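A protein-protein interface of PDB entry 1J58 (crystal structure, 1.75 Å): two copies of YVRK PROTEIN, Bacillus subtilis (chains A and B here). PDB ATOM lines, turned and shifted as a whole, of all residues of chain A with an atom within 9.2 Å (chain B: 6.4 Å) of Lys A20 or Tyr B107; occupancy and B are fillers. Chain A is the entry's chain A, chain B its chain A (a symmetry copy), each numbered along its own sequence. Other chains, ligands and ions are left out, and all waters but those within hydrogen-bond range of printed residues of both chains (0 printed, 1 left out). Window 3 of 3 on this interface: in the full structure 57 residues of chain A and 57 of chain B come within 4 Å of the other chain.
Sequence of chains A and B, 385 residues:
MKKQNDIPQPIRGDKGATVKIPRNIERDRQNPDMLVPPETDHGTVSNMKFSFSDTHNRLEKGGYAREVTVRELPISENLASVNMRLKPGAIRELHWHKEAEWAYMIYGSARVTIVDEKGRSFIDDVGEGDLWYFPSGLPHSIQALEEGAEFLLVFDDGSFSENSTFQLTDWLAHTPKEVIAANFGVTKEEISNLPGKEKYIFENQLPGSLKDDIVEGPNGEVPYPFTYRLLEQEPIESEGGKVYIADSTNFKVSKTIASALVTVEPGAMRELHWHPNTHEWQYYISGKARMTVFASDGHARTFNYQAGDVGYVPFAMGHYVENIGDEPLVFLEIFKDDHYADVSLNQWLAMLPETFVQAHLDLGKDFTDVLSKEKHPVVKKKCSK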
ATOM      1  N   PRO A   8      32.136  12.696  24.481  1.00  0.00           N
ATOM      2  CA  PRO A   8      31.139  11.982  25.312  1.00  0.00           C
ATOM      3  C   PRO A   8      30.147  11.223  24.436  1.00  0.00           C
ATOM      4  O   PRO A   8      29.884  11.618  23.302  1.00  0.00           O
ATOM      5  CB  PRO A   8      30.425  13.043  26.135  1.00  0.00           C
ATOM      6  CG  PRO A   8      30.512  14.241  25.198  1.00  0.00           C
ATOM      7  CD  PRO A   8      31.927  14.151  24.593  1.00  0.00           C
ATOM      8  N   GLN A   9      29.603  10.132  24.966  1.00  0.00           N
ATOM      9  CA  GLN A   9      28.632   9.322  24.240  1.00  0.00           C
ATOM     10  C   GLN A   9      27.428   9.002  25.124  1.00  0.00           C
ATOM     11  O   GLN A   9      27.563   8.816  26.337  1.00  0.00           O
ATOM     12  CB  GLN A   9      29.269   8.008  23.775  1.00  0.00           C
ATOM     13  CG  GLN A   9      30.405   8.163  22.770  1.00  0.00           C
ATOM     14  CD  GLN A   9      29.935   8.682  21.425  1.00  0.00           C
ATOM     15  OE1 GLN A   9      28.735   8.810  21.179  1.00  0.00           O
ATOM     16  NE2 GLN A   9      30.880   8.976  20.540  1.00  0.00           N
ATOM     17  N   PRO A  10      26.229   8.934  24.525  1.00  0.00           N
ATOM     18  CA  PRO A  10      25.021   8.628  25.296  1.00  0.00           C
ATOM     19  C   PRO A  10      24.953   7.138  25.635  1.00  0.00           C
ATOM     20  O   PRO A  10      24.135   6.392  25.095  1.00  0.00           O
ATOM     21  CB  PRO A  10      23.897   9.091  24.372  1.00  0.00           C
ATOM     22  CG  PRO A  10      24.462   8.842  23.008  1.00  0.00           C
ATOM     23  CD  PRO A  10      25.898   9.293  23.133  1.00  0.00           C
ATOM     24  N   ALA A  17      24.054   4.095  23.079  1.00  0.00           N
ATOM     25  CA  ALA A  17      24.961   3.769  21.984  1.00  0.00           C
ATOM     26  C   ALA A  17      25.706   5.025  21.554  1.00  0.00           C
ATOM     27  O   ALA A  17      25.377   6.129  21.983  1.00  0.00           O
ATOM     28  CB  ALA A  17      24.167   3.212  20.807  1.00  0.00           C
ATOM     29  N   THR A  18      26.715   4.860  20.706  1.00  0.00           N
ATOM     30  CA  THR A  18      27.470   6.009  20.225  1.00  0.00           C
ATOM     31  C   THR A  18      26.610   6.781  19.231  1.00  0.00           C
ATOM     32  O   THR A  18      25.716   6.211  18.605  1.00  0.00           O
ATOM     33  CB  THR A  18      28.763   5.574  19.508  1.00  0.00           C
ATOM     34  OG1 THR A  18      28.437   4.661  18.451  1.00  0.00           O
ATOM     35  CG2 THR A  18      29.718   4.905  20.490  1.00  0.00           C
ATOM     36  N   VAL A  19      26.868   8.081  19.101  1.00  0.00           N
ATOM     37  CA  VAL A  19      26.126   8.906  18.153  1.00  0.00           C
ATOM     38  C   VAL A  19      26.781   8.687  16.793  1.00  0.00           C
ATOM     39  O   VAL A  19      27.995   8.815  16.662  1.00  0.00           O
ATOM     40  CB  VAL A  19      26.208  10.403  18.522  1.00  0.00           C
ATOM     41  CG1 VAL A  19      25.454  11.231  17.490  1.00  0.00           C
ATOM     42  CG2 VAL A  19      25.619  10.629  19.911  1.00  0.00           C
ATOM     43  N   LYS A  20      25.976   8.360  15.786  1.00  0.00           N
ATOM     44  CA  LYS A  20      26.497   8.092  14.448  1.00  0.00           C
ATOM     45  C   LYS A  20      26.294   9.227  13.448  1.00  0.00           C
ATOM     46  O   LYS A  20      26.905   9.228  12.381  1.00  0.00           O
ATOM     47  CB  LYS A  20      25.856   6.817  13.887  1.00  0.00           C
ATOM     48  CG  LYS A  20      26.281   5.534  14.588  1.00  0.00           C
ATOM     49  CD  LYS A  20      27.717   5.161  14.239  1.00  0.00           C
ATOM     50  CE  LYS A  20      28.104   3.826  14.864  1.00  0.00           C
ATOM     51  NZ  LYS A  20      29.496   3.432  14.492  1.00  0.00           N
ATOM     52  N   ILE A  21      25.442  10.185  13.783  1.00  0.00           N
ATOM     53  CA  ILE A  21      25.174  11.300  12.878  1.00  0.00           C
ATOM     54  C   ILE A  21      25.903  12.572  13.304  1.00  0.00           C
ATOM     55  O   ILE A  21      26.440  12.649  14.410  1.00  0.00           O
ATOM     56  CB  ILE A  21      23.656  11.607  12.813  1.00  0.00           C
ATOM     57  CG1 ILE A  21      23.158  12.061  14.186  1.00  0.00           C
ATOM     58  CG2 ILE A  21      22.886  10.365  12.370  1.00  0.00           C
ATOM     59  CD1 ILE A  21      21.679  12.434  14.220  1.00  0.00           C
ATOM     60  N   PRO A  22      25.958  13.580  12.417  1.00  0.00           N
ATOM     61  CA  PRO A  22      26.635  14.829  12.778  1.00  0.00           C
ATOM     62  C   PRO A  22      25.976  15.358  14.053  1.00  0.00           C
ATOM     63  O   PRO A  22      24.753  15.320  14.188  1.00  0.00           O
ATOM     64  CB  PRO A  22      26.384  15.715  11.562  1.00  0.00           C
ATOM     65  CG  PRO A  22      26.403  14.723  10.435  1.00  0.00           C
ATOM     66  CD  PRO A  22      25.554  13.593  10.998  1.00  0.00           C
ATOM     67  N   ARG A  23      26.786  15.854  14.982  1.00  0.00           N
ATOM     68  CA  ARG A  23      26.267  16.308  16.266  1.00  0.00           C
ATOM     69  C   ARG A  23      26.902  17.595  16.781  1.00  0.00           C
ATOM     70  O   ARG A  23      27.856  18.115  16.204  1.00  0.00           O
ATOM     71  CB  ARG A  23      26.501  15.204  17.293  1.00  0.00           C
ATOM     72  CG  ARG A  23      27.982  14.863  17.410  1.00  0.00           C
ATOM     73  CD  ARG A  23      28.259  13.616  18.226  1.00  0.00           C
ATOM     74  NE  ARG A  23      27.866  13.769  19.619  1.00  0.00           N
ATOM     75  CZ  ARG A  23      28.334  13.011  20.604  1.00  0.00           C
ATOM     76  NH1 ARG A  23      29.214  12.053  20.342  1.00  0.00           N
ATOM     77  NH2 ARG A  23      27.920  13.209  21.848  1.00  0.00           N
ATOM     78  N   TYR B  64      18.833   4.583  21.643  1.00  0.00           N
ATOM     79  CA  TYR B  64      18.337   5.749  22.362  1.00  0.00           C
ATOM     80  C   TYR B  64      17.339   6.560  21.545  1.00  0.00           C
ATOM     81  O   TYR B  64      17.162   6.335  20.349  1.00  0.00           O
ATOM     82  CB  TYR B  64      19.501   6.650  22.817  1.00  0.00           C
ATOM     83  CG  TYR B  64      20.356   7.263  21.718  1.00  0.00           C
ATOM     84  CD1 TYR B  64      19.847   8.244  20.863  1.00  0.00           C
ATOM     85  CD2 TYR B  64      21.689   6.883  21.559  1.00  0.00           C
ATOM     86  CE1 TYR B  64      20.648   8.832  19.876  1.00  0.00           C
ATOM     87  CE2 TYR B  64      22.498   7.465  20.576  1.00  0.00           C
ATOM     88  CZ  TYR B  64      21.969   8.435  19.740  1.00  0.00           C
ATOM     89  OH  TYR B  64      22.762   8.998  18.764  1.00  0.00           O
ATOM     90  N   ARG B  85      18.126   6.137  17.624  1.00  0.00           N
ATOM     91  CA  ARG B  85      19.323   5.361  17.316  1.00  0.00           C
ATOM     92  C   ARG B  85      19.081   3.903  17.710  1.00  0.00           C
ATOM     93  O   ARG B  85      18.559   3.621  18.791  1.00  0.00           O
ATOM     94  CB  ARG B  85      20.503   5.914  18.120  1.00  0.00           C
ATOM     95  CG  ARG B  85      21.818   6.093  17.357  1.00  0.00           C
ATOM     96  CD  ARG B  85      22.375   4.785  16.869  1.00  0.00           C
ATOM     97  NE  ARG B  85      23.810   4.653  17.119  1.00  0.00           N
ATOM     98  CZ  ARG B  85      24.493   3.538  16.886  1.00  0.00           C
ATOM     99  NH1 ARG B  85      23.867   2.477  16.392  1.00  0.00           N
ATOM    100  NH2 ARG B  85      25.786   3.468  17.168  1.00  0.00           N
ATOM    101  N   LEU B  86      19.455   2.978  16.831  1.00  0.00           N
ATOM    102  CA  LEU B  86      19.298   1.554  17.113  1.00  0.00           C
ATOM    103  C   LEU B  86      20.603   0.831  16.810  1.00  0.00           C
ATOM    104  O   LEU B  86      21.237   1.088  15.789  1.00  0.00           O
ATOM    105  CB  LEU B  86      18.177   0.943  16.263  1.00  0.00           C
ATOM    106  CG  LEU B  86      16.726   1.318  16.578  1.00  0.00           C
ATOM    107  CD1 LEU B  86      15.792   0.628  15.582  1.00  0.00           C
ATOM    108  CD2 LEU B  86      16.386   0.900  18.001  1.00  0.00           C
ATOM    109  N   TYR B 104      13.495   9.880   7.890  1.00  0.00           N
ATOM    110  CA  TYR B 104      14.621  10.004   6.970  1.00  0.00           C
ATOM    111  C   TYR B 104      15.779   9.225   7.595  1.00  0.00           C
ATOM    112  O   TYR B 104      16.168   9.498   8.733  1.00  0.00           O
ATOM    113  CB  TYR B 104      15.026  11.473   6.809  1.00  0.00           C
ATOM    114  CG  TYR B 104      16.217  11.667   5.899  1.00  0.00           C
ATOM    115  CD1 TYR B 104      16.071  11.637   4.517  1.00  0.00           C
ATOM    116  CD2 TYR B 104      17.498  11.838   6.422  1.00  0.00           C
ATOM    117  CE1 TYR B 104      17.171  11.774   3.671  1.00  0.00           C
ATOM    118  CE2 TYR B 104      18.607  11.974   5.585  1.00  0.00           C
ATOM    119  CZ  TYR B 104      18.432  11.940   4.213  1.00  0.00           C
ATOM    120  OH  TYR B 104      19.517  12.071   3.375  1.00  0.00           O
ATOM    121  N   MET B 105      16.318   8.250   6.867  1.00  0.00           N
ATOM    122  CA  MET B 105      17.431   7.448   7.372  1.00  0.00           C
ATOM    123  C   MET B 105      18.734   8.207   7.146  1.00  0.00           C
ATOM    124  O   MET B 105      19.181   8.367   6.008  1.00  0.00           O
ATOM    125  CB  MET B 105      17.484   6.097   6.644  1.00  0.00           C
ATOM    126  CG  MET B 105      18.573   5.136   7.138  1.00  0.00           C
ATOM    127  SD  MET B 105      18.315   4.509   8.972  1.00  0.00           S
ATOM    128  CE  MET B 105      16.461   4.037   8.816  1.00  0.00           C
ATOM    129  N   ILE B 106      19.343   8.678   8.228  1.00  0.00           N
ATOM    130  CA  ILE B 106      20.586   9.437   8.119  1.00  0.00           C
ATOM    131  C   ILE B 106      21.792   8.514   8.065  1.00  0.00           C
ATOM    132  O   ILE B 106      22.709   8.708   7.259  1.00  0.00           O
ATOM    133  CB  ILE B 106      20.764  10.389   9.317  1.00  0.00           C
ATOM    134  CG1 ILE B 106      19.551  11.317   9.435  1.00  0.00           C
ATOM    135  CG2 ILE B 106      22.037  11.209   9.142  1.00  0.00           C
ATOM    136  CD1 ILE B 106      19.526  12.126  10.724  1.00  0.00           C
ATOM    137  N   TYR B 107      21.782   7.507   8.931  1.00  0.00           N
ATOM    138  CA  TYR B 107      22.876   6.551   9.014  1.00  0.00           C
ATOM    139  C   TYR B 107      22.393   5.110   9.089  1.00  0.00           C
ATOM    140  O   TYR B 107      21.381   4.814   9.720  1.00  0.00           O
ATOM    141  CB  TYR B 107      23.732   6.835  10.254  1.00  0.00           C
ATOM    142  CG  TYR B 107      24.650   5.687  10.622  1.00  0.00           C
ATOM    143  CD1 TYR B 107      25.893   5.539  10.009  1.00  0.00           C
ATOM    144  CD2 TYR B 107      24.244   4.710  11.533  1.00  0.00           C
ATOM    145  CE1 TYR B 107      26.708   4.443  10.290  1.00  0.00           C
ATOM    146  CE2 TYR B 107      25.052   3.608  11.820  1.00  0.00           C
ATOM    147  CZ  TYR B 107      26.280   3.480  11.192  1.00  0.00           C
ATOM    148  OH  TYR B 107      27.067   2.378  11.447  1.00  0.00           O
ATOM    149  N   GLY B 108      23.137   4.215   8.450  1.00  0.00           N
ATOM    150  CA  GLY B 108      22.805   2.804   8.494  1.00  0.00           C
ATOM    151  C   GLY B 108      21.623   2.339   7.672  1.00  0.00           C
ATOM    152  O   GLY B 108      21.361   2.840   6.580  1.00  0.00           O
ATOM    153  N   SER B 109      20.914   1.352   8.206  1.00  0.00           N
ATOM    154  CA  SER B 109      19.758   0.795   7.525  1.00  0.00           C
ATOM    155  C   SER B 109      18.889   0.058   8.528  1.00  0.00           C
ATOM    156  O   SER B 109      19.330  -0.266   9.631  1.00  0.00           O
ATOM    157  CB  SER B 109      20.206  -0.162   6.417  1.00  0.00           C
ATOM    158  OG  SER B 109      20.997  -1.218   6.936  1.00  0.00           O
ATOM    159  N   GLY B 127      17.549   2.212   3.555  1.00  0.00           N
ATOM    160  CA  GLY B 127      18.945   2.590   3.689  1.00  0.00           C
ATOM    161  C   GLY B 127      19.133   4.091   3.790  1.00  0.00           C
ATOM    162  O   GLY B 127      18.157   4.849   3.795  1.00  0.00           O
ATOM    163  N   GLU B 128      20.387   4.524   3.872  1.00  0.00           N
ATOM    164  CA  GLU B 128      20.689   5.948   3.975  1.00  0.00           C
ATOM    165  C   GLU B 128      20.099   6.715   2.800  1.00  0.00           C
ATOM    166  O   GLU B 128      20.296   6.348   1.644  1.00  0.00           O
ATOM    167  CB  GLU B 128      22.207   6.164   4.042  1.00  0.00           C
ATOM    168  CG  GLU B 128      22.824   5.713   5.359  1.00  0.00           C
ATOM    169  CD  GLU B 128      24.345   5.741   5.352  1.00  0.00           C
ATOM    170  OE1 GLU B 128      24.933   6.253   4.373  1.00  0.00           O
ATOM    171  OE2 GLU B 128      24.951   5.255   6.333  1.00  0.00           O
ATOM    172  N   GLY B 129      19.363   7.779   3.108  1.00  0.00           N
ATOM    173  CA  GLY B 129      18.749   8.583   2.070  1.00  0.00           C
ATOM    174  C   GLY B 129      17.318   8.176   1.766  1.00  0.00           C
ATOM    175  O   GLY B 129      16.629   8.857   1.005  1.00  0.00           O
ATOM    176  N   GLU B 146      22.801  -4.800  10.071  1.00  0.00           N
ATOM    177  CA  GLU B 146      24.177  -4.948  10.545  1.00  0.00           C
ATOM    178  C   GLU B 146      25.017  -3.715  10.864  1.00  0.00           C
ATOM    179  O   GLU B 146      26.001  -3.815  11.593  1.00  0.00           O
ATOM    180  CB  GLU B 146      24.961  -5.873   9.596  1.00  0.00           C
ATOM    181  CG  GLU B 146      25.365  -5.288   8.246  1.00  0.00           C
ATOM    182  CD  GLU B 146      24.203  -5.087   7.295  1.00  0.00           C
ATOM    183  OE1 GLU B 146      23.183  -5.802   7.413  1.00  0.00           O
ATOM    184  OE2 GLU B 146      24.323  -4.217   6.405  1.00  0.00           O
ATOM    185  N   GLU B 147      24.648  -2.556  10.333  1.00  0.00           N
ATOM    186  CA  GLU B 147      25.406  -1.341  10.611  1.00  0.00           C
ATOM    187  C   GLU B 147      24.735  -0.536  11.718  1.00  0.00           C
ATOM    188  O   GLU B 147      25.273   0.473  12.181  1.00  0.00           O
ATOM    189  CB  GLU B 147      25.498  -0.469   9.354  1.00  0.00           C
ATOM    190  CG  GLU B 147      26.350  -1.042   8.221  1.00  0.00           C
ATOM    191  CD  GLU B 147      27.807  -1.221   8.616  1.00  0.00           C
ATOM    192  OE1 GLU B 147      28.305  -0.416   9.423  1.00  0.00           O
ATOM    193  OE2 GLU B 147      28.460  -2.156   8.107  1.00  0.00           O
ATOM    194  N   GLY B 148      23.573  -1.003  12.156  1.00  0.00           N
ATOM    195  CA  GLY B 148      22.832  -0.269  13.161  1.00  0.00           C
ATOM    196  C   GLY B 148      22.093   0.799  12.375  1.00  0.00           C
ATOM    197  O   GLY B 148      22.076   0.756  11.141  1.00  0.00           O
ATOM    198  N   ALA B 149      21.491   1.765  13.059  1.00  0.00           N
ATOM    199  CA  ALA B 149      20.769   2.809  12.352  1.00  0.00           C
ATOM    200  C   ALA B 149      20.501   4.034  13.212  1.00  0.00           C
ATOM    201  O   ALA B 149      20.369   3.935  14.427  1.00  0.00           O
ATOM    202  CB  ALA B 149      19.440   2.253  11.836  1.00  0.00           C
ATOM    203  N   GLU B 150      20.453   5.196  12.574  1.00  0.00           N
ATOM    204  CA  GLU B 150      20.118   6.427  13.276  1.00  0.00           C
ATOM    205  C   GLU B 150      19.317   7.242  12.280  1.00  0.00           C
ATOM    206  O   GLU B 150      19.755   7.489  11.153  1.00  0.00           O
ATOM    207  CB  GLU B 150      21.359   7.186  13.756  1.00  0.00           C
ATOM    208  CG  GLU B 150      20.982   8.453  14.524  1.00  0.00           C
ATOM    209  CD  GLU B 150      22.000   8.857  15.570  1.00  0.00           C
ATOM    210  OE1 GLU B 150      23.170   8.430  15.469  1.00  0.00           O
ATOM    211  OE2 GLU B 150      21.625   9.609  16.498  1.00  0.00           O
ATOM    212  N   PHE B 151      18.131   7.654  12.701  1.00  0.00           N
ATOM    213  CA  PHE B 151      17.234   8.365  11.812  1.00  0.00           C
ATOM    214  C   PHE B 151      16.424   9.449  12.498  1.00  0.00           C
ATOM    215  O   PHE B 151      16.376   9.537  13.729  1.00  0.00           O
ATOM    216  CB  PHE B 151      16.299   7.337  11.161  1.00  0.00           C
ATOM    217  CG  PHE B 151      15.791   6.287  12.120  1.00  0.00           C
ATOM    218  CD1 PHE B 151      14.561   6.432  12.754  1.00  0.00           C
ATOM    219  CD2 PHE B 151      16.563   5.162  12.413  1.00  0.00           C
ATOM    220  CE1 PHE B 151      14.105   5.477  13.662  1.00  0.00           C
ATOM    221  CE2 PHE B 151      16.117   4.198  13.320  1.00  0.00           C
ATOM    222  CZ  PHE B 151      14.884   4.356  13.947  1.00  0.00           C
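The backbone carbonyl oxygen (O) of Thr A18 sits at hydrogen-bond distance from the guanidinium group (NE) of Arg B85 (2.9 Å).
OE1 of Glu B150 is in hydrogen-bond range of N of Lys A20 (2.8 Å).
OE1 of Glu B150 lies within hydrogen-bond range of N of Ile A21, at 3.3 Å.
N of Arg B85 is in hydrogen-bond range of O of Tyr B64 (2.9 Å).
OE2 of Glu B150 sits at hydrogen-bond distance from OH of Tyr B64 (2.6 Å).
N of Ile B106 is in hydrogen-bond range of O of Glu B150, at 3.2 Å.
OE1 of Gln A9 sits at hydrogen-bond distance from N of Val A19 (2.9 Å).
O of Glu B150 lies within hydrogen-bond range of N of Tyr B107.
The backbone carbonyl oxygen (O) of Pro A10 is in hydrogen-bond range of the backbone NH (N) of Ala A17 (3.1 Å).
Pro A10 touches Tyr B64 (CG to CE2, 3.4 Å).
Tyr B64 touches Ala A17 (CE2 to O, 3.5 Å).
CB of Ala A17 touches CZ of Arg B85 (3.9 Å).
Thr A18 touches Tyr B64.
CA of Val A19 touches OH of Tyr B64 (3.4 Å).
OE1 of Glu B150 touches C of Val A19, at 3.9 Å.
Lys A20 touches Arg B85 (CE to NH2, 3.3 Å).
Lys A20 touches Tyr B107.
Ile A21 touches Ile B106 (CG2 to CG2, 3.4 Å).
Of chain B, only Arg B85, Tyr B107 and Glu B150 come within 4 Å of Lys A20.
No residue of chain A comes within 4 Å of Gly B148.
No residue of chain A comes within 4 Å of Ala B149.
Of the printed residues of chain A, Tyr B64 touches Pro A10, Ala A17, Thr A18 and Val A19.
Of the printed residues of chain B, Thr A18 touches Tyr B64 (3.98 Å) and Arg B85 (2.9 Å).
Of the printed residues of chain B, Val A19 touches Tyr B64 and Glu B150.
Of the printed residues of chain B, Pro A10 touches Tyr B64 (3.4 Å).
Leu B86 touches none of the printed residues of chain A.
The nearest residue of chain A that does not touch Tyr B107 is Ile A21 (4.2 Å).
Hydrophobic or aromatic side chains of chain B within 4 Å of the printed part of chain A: Tyr B64, Ile B106 and Tyr B107.
Printed residues of chain A that touch a printed residue of chain B: Pro A10, Ala A17, Thr A18, Val A19, Lys A20 and Ile A21.
Hydrophobic or aromatic side chains of chain A that line the printed part of chain B: Pro A10, Ala A17, Val A19 and Ile A21.
Among the printed residues, no Asp or Glu carboxylate lies within 4 Å of a Lys or Arg side-chain nitrogen of the other chain.
No position is printed for both chains.
Of the 12 pairs that touch across the chains among the printed residues, none has its exchanged pair printed and touching as well.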
